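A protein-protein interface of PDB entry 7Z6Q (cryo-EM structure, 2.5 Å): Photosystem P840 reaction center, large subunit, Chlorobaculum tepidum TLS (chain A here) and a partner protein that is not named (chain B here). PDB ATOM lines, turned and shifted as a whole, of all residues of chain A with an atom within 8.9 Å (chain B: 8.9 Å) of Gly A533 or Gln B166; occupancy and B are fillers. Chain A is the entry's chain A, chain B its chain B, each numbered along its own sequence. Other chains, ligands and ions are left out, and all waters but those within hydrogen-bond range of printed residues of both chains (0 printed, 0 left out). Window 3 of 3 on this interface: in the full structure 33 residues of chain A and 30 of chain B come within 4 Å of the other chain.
Hydrophobic or aromatic side chains of chain A that line the printed part of chain B: Pro A530 and Val A531. Along chain A the printed residues that touch a printed residue of chain B span positions 530 to 533. Of the 9 printed residues of chain B, 4 touch a printed residue of chain A. Printed residues of chain B that touch a printed residue of chain A: Val B141, Val B165, Gln B166 and Phe B170. Along chain B the printed residues that touch a printed residue of chain A span positions 141 to 170. Among the printed residues, 8 pairs touch across the chains. Among the printed residues, no Asp or Glu carboxylate lies within 4 Å of a Lys or Arg side-chain nitrogen of the other chain.
O of Gln B166 lies within hydrogen-bond range of N of Gly A533, 3.3 Å away.
Among the printed residues, merely in contact across the chains: Pro A530 with Val B165 (3.3 Å), Pro A530 with Gln B166 (3.6 Å), Pro A530 with Phe B170 (3.1 Å), Val A531 with Val B141 (2.8 Å), Val A531 with Val B165 (3.5 Å), Val A531 with Phe B170 (3.9 Å) and Tyr A532 with Gln B166 (3.8 Å).
Printed residues of chain B within 4 Å of Pro A530: Val B165, Gln B166 and Phe B170. Printed residues of chain B within 4 Å of Val A531: Val B141, Val B165 and Phe B170. Printed residues of chain B within 4 Å of Tyr A532: Gln B166 (3.8 Å). Printed residues of chain B within 4 Å of Gly A533: Gln B166 (3.3 Å). No residue of chain B comes within 4 Å of Gly A534. Of the printed residues of chain A, Val B141 touches Val A531 (2.8 Å). Of chain A, only Pro A530 and Val A531 come within 4 Å of Val B165. Gln B166 touches just these residues of chain A: Pro A530, Tyr A532 and Gly A533. Of the printed residues of chain A, Phe B170 touches Pro A530 (3.1 Å) and Val A531 (3.9 Å). The nearest residue of chain B that does not touch Gly A533 is Glu B167 (5.5 Å).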
ATOM      1  N   LEU A 516      27.281  27.523  -2.773  1.00  0.00           N
ATOM      2  CA  LEU A 516      26.427  26.636  -3.554  1.00  0.00           C
ATOM      3  C   LEU A 516      26.624  25.176  -3.171  1.00  0.00           C
ATOM      4  O   LEU A 516      26.015  24.287  -3.775  1.00  0.00           O
ATOM      5  CB  LEU A 516      26.682  26.817  -5.052  1.00  0.00           C
ATOM      6  CG  LEU A 516      26.420  28.202  -5.641  1.00  0.00           C
ATOM      7  CD1 LEU A 516      26.488  28.148  -7.157  1.00  0.00           C
ATOM      8  CD2 LEU A 516      25.073  28.730  -5.180  1.00  0.00           C
ATOM      9  N   GLY A 529      27.689  21.893 -15.810  1.00  0.00           N
ATOM     10  CA  GLY A 529      26.464  21.734 -16.613  1.00  0.00           C
ATOM     11  C   GLY A 529      25.620  22.996 -16.609  1.00  0.00           C
ATOM     12  O   GLY A 529      26.089  24.018 -16.077  1.00  0.00           O
ATOM     13  N   PRO A 530      24.379  22.953 -17.140  1.00  0.00           N
ATOM     14  CA  PRO A 530      23.500  24.128 -17.233  1.00  0.00           C
ATOM     15  C   PRO A 530      23.103  24.738 -15.882  1.00  0.00           C
ATOM     16  O   PRO A 530      22.855  25.923 -15.834  1.00  0.00           O
ATOM     17  CB  PRO A 530      22.269  23.619 -17.992  1.00  0.00           C
ATOM     18  CG  PRO A 530      22.285  22.129 -17.773  1.00  0.00           C
ATOM     19  CD  PRO A 530      23.747  21.757 -17.686  1.00  0.00           C
ATOM     20  N   VAL A 531      23.053  23.907 -14.837  1.00  0.00           N
ATOM     21  CA  VAL A 531      22.674  24.241 -13.426  1.00  0.00           C
ATOM     22  C   VAL A 531      23.192  25.612 -12.953  1.00  0.00           C
ATOM     23  O   VAL A 531      24.378  25.926 -13.207  1.00  0.00           O
ATOM     24  CB  VAL A 531      23.129  23.118 -12.473  1.00  0.00           C
ATOM     25  CG1 VAL A 531      22.418  21.804 -12.759  1.00  0.00           C
ATOM     26  CG2 VAL A 531      24.638  22.932 -12.493  1.00  0.00           C
ATOM     27  N   TYR A 532      22.366  26.296 -12.149  1.00  0.00           N
ATOM     28  CA  TYR A 532      22.666  27.632 -11.567  1.00  0.00           C
ATOM     29  C   TYR A 532      22.990  28.606 -12.701  1.00  0.00           C
ATOM     30  O   TYR A 532      24.053  29.258 -12.668  1.00  0.00           O
ATOM     31  CB  TYR A 532      23.768  27.553 -10.506  1.00  0.00           C
ATOM     32  CG  TYR A 532      23.444  26.685  -9.317  1.00  0.00           C
ATOM     33  CD1 TYR A 532      22.693  27.172  -8.260  1.00  0.00           C
ATOM     34  CD2 TYR A 532      23.886  25.375  -9.245  1.00  0.00           C
ATOM     35  CE1 TYR A 532      22.390  26.382  -7.164  1.00  0.00           C
ATOM     36  CE2 TYR A 532      23.592  24.571  -8.157  1.00  0.00           C
ATOM     37  CZ  TYR A 532      22.840  25.075  -7.112  1.00  0.00           C
ATOM     38  OH  TYR A 532      22.546  24.290  -6.034  1.00  0.00           O
ATOM     39  N   GLY A 533      22.107  28.685 -13.702  1.00  0.00           N
ATOM     40  CA  GLY A 533      22.361  29.563 -14.862  1.00  0.00           C
ATOM     41  C   GLY A 533      23.626  29.133 -15.586  1.00  0.00           C
ATOM     42  O   GLY A 533      24.048  29.838 -16.523  1.00  0.00           O
ATOM     43  N   GLY A 534      24.207  28.008 -15.156  1.00  0.00           N
ATOM     44  CA  GLY A 534      25.444  27.464 -15.750  1.00  0.00           C
ATOM     45  C   GLY A 534      26.668  27.873 -14.948  1.00  0.00           C
ATOM     46  O   GLY A 534      26.704  28.882 -14.189  1.00  0.00           O
ATOM     47  N   THR A 535      27.749  27.092 -15.049  1.00  0.00           N
ATOM     48  CA  THR A 535      29.011  27.378 -14.312  1.00  0.00           C
ATOM     49  C   THR A 535      30.208  26.969 -15.177  1.00  0.00           C
ATOM     50  O   THR A 535      31.039  26.175 -14.693  1.00  0.00           O
ATOM     51  CB  THR A 535      29.054  26.636 -12.969  1.00  0.00           C
ATOM     52  OG1 THR A 535      28.735  25.265 -13.212  1.00  0.00           O
ATOM     53  CG2 THR A 535      28.104  27.207 -11.940  1.00  0.00           C
ATOM     54  N   CYS A 536      30.285  27.491 -16.406  1.00  0.00           N
ATOM     55  CA  CYS A 536      31.383  27.163 -17.304  1.00  0.00           C
ATOM     56  C   CYS A 536      32.625  27.998 -17.010  1.00  0.00           C
ATOM     57  O   CYS A 536      32.545  29.134 -16.541  1.00  0.00           O
ATOM     58  CB  CYS A 536      30.957  27.372 -18.755  1.00  0.00           C
ATOM     59  SG  CYS A 536      29.651  26.265 -19.324  1.00  0.00           S
ATOM     60  N   GLU A 633      30.350  27.827 -27.210  1.00  0.00           N
ATOM     61  CA  GLU A 633      29.586  26.769 -26.493  1.00  0.00           C
ATOM     62  C   GLU A 633      28.772  25.940 -27.489  1.00  0.00           C
ATOM     63  O   GLU A 633      27.538  26.009 -27.436  1.00  0.00           O
ATOM     64  CB  GLU A 633      28.665  27.432 -25.470  1.00  0.00           C
ATOM     65  CG  GLU A 633      29.414  28.098 -24.337  1.00  0.00           C
ATOM     66  CD  GLU A 633      28.759  29.365 -23.829  1.00  0.00           C
ATOM     67  OE1 GLU A 633      27.850  29.861 -24.510  1.00  0.00           O
ATOM     68  OE2 GLU A 633      29.166  29.857 -22.760  1.00  0.00           O
ATOM     69  N   VAL B 141      23.533  17.766  -9.411  1.00  0.00           N
ATOM     70  CA  VAL B 141      23.393  18.856 -10.360  1.00  0.00           C
ATOM     71  C   VAL B 141      23.378  18.348 -11.793  1.00  0.00           C
ATOM     72  O   VAL B 141      23.382  19.143 -12.730  1.00  0.00           O
ATOM     73  CB  VAL B 141      24.491  19.919 -10.158  1.00  0.00           C
ATOM     74  CG1 VAL B 141      24.510  20.387  -8.714  1.00  0.00           C
ATOM     75  CG2 VAL B 141      25.846  19.362 -10.555  1.00  0.00           C
ATOM     76  N   GLY B 163      12.184  19.525 -16.010  1.00  0.00           N
ATOM     77  CA  GLY B 163      12.096  20.998 -16.098  1.00  0.00           C
ATOM     78  C   GLY B 163      13.208  21.609 -16.934  1.00  0.00           C
ATOM     79  O   GLY B 163      13.835  20.864 -17.704  1.00  0.00           O
ATOM     80  N   ASP B 164      13.403  22.928 -16.828  1.00  0.00           N
ATOM     81  CA  ASP B 164      14.495  23.610 -17.575  1.00  0.00           C
ATOM     82  C   ASP B 164      15.827  23.361 -16.857  1.00  0.00           C
ATOM     83  O   ASP B 164      15.928  23.696 -15.666  1.00  0.00           O
ATOM     84  CB  ASP B 164      14.201  25.091 -17.828  1.00  0.00           C
ATOM     85  CG  ASP B 164      14.138  25.910 -16.557  1.00  0.00           C
ATOM     86  OD1 ASP B 164      13.739  25.359 -15.509  1.00  0.00           O
ATOM     87  OD2 ASP B 164      14.491  27.086 -16.633  1.00  0.00           O
ATOM     88  N   VAL B 165      16.839  22.945 -17.623  1.00  0.00           N
ATOM     89  CA  VAL B 165      18.193  22.545 -17.142  1.00  0.00           C
ATOM     90  C   VAL B 165      18.870  23.695 -16.389  1.00  0.00           C
ATOM     91  O   VAL B 165      19.614  23.398 -15.450  1.00  0.00           O
ATOM     92  CB  VAL B 165      19.055  22.019 -18.305  1.00  0.00           C
ATOM     93  CG1 VAL B 165      18.487  20.734 -18.887  1.00  0.00           C
ATOM     94  CG2 VAL B 165      19.232  23.064 -19.391  1.00  0.00           C
ATOM     95  N   GLN B 166      18.621  24.940 -16.809  1.00  0.00           N
ATOM     96  CA  GLN B 166      19.233  26.132 -16.162  1.00  0.00           C
ATOM     97  C   GLN B 166      18.657  26.298 -14.751  1.00  0.00           C
ATOM     98  O   GLN B 166      19.189  27.132 -13.991  1.00  0.00           O
ATOM     99  CB  GLN B 166      18.982  27.383 -17.008  1.00  0.00           C
ATOM    100  CG  GLN B 166      19.981  27.564 -18.141  1.00  0.00           C
ATOM    101  CD  GLN B 166      19.766  28.854 -18.892  1.00  0.00           C
ATOM    102  OE1 GLN B 166      18.739  29.514 -18.749  1.00  0.00           O
ATOM    103  NE2 GLN B 166      20.741  29.227 -19.704  1.00  0.00           N
ATOM    104  N   GLU B 167      17.613  25.531 -14.424  1.00  0.00           N
ATOM    105  CA  GLU B 167      16.970  25.609 -13.085  1.00  0.00           C
ATOM    106  C   GLU B 167      17.043  24.239 -12.402  1.00  0.00           C
ATOM    107  O   GLU B 167      16.054  23.856 -11.745  1.00  0.00           O
ATOM    108  CB  GLU B 167      15.520  26.077 -13.220  1.00  0.00           C
ATOM    109  CG  GLU B 167      15.061  26.961 -12.074  1.00  0.00           C
ATOM    110  CD  GLU B 167      15.459  28.421 -12.203  1.00  0.00           C
ATOM    111  OE1 GLU B 167      15.158  29.023 -13.253  1.00  0.00           O
ATOM    112  OE2 GLU B 167      16.068  28.952 -11.253  1.00  0.00           O
ATOM    113  N   GLY B 168      18.170  23.536 -12.554  1.00  0.00           N
ATOM    114  CA  GLY B 168      18.336  22.211 -11.931  1.00  0.00           C
ATOM    115  C   GLY B 168      17.175  21.301 -12.282  1.00  0.00           C
ATOM    116  O   GLY B 168      16.711  20.581 -11.397  1.00  0.00           O
ATOM    117  N   GLY B 169      16.751  21.308 -13.543  1.00  0.00           N
ATOM    118  CA  GLY B 169      15.615  20.494 -14.012  1.00  0.00           C
ATOM    119  C   GLY B 169      16.000  19.069 -14.362  1.00  0.00           C
ATOM    120  O   GLY B 169      15.127  18.351 -14.852  1.00  0.00           O
ATOM    121  N   PHE B 170      17.253  18.675 -14.144  1.00  0.00           N
ATOM    122  CA  PHE B 170      17.676  17.299 -14.517  1.00  0.00           C
ATOM    123  C   PHE B 170      18.595  16.718 -13.441  1.00  0.00           C
ATOM    124  O   PHE B 170      19.298  17.482 -12.764  1.00  0.00           O
ATOM    125  CB  PHE B 170      18.312  17.282 -15.909  1.00  0.00           C
ATOM    126  CG  PHE B 170      19.633  18.000 -16.017  1.00  0.00           C
ATOM    127  CD1 PHE B 170      19.718  19.368 -15.822  1.00  0.00           C
ATOM    128  CD2 PHE B 170      20.789  17.303 -16.310  1.00  0.00           C
ATOM    129  CE1 PHE B 170      20.933  20.023 -15.911  1.00  0.00           C
ATOM    130  CE2 PHE B 170      22.001  17.961 -16.412  1.00  0.00           C
ATOM    131  CZ  PHE B 170      22.068  19.316 -16.211  1.00  0.00           C
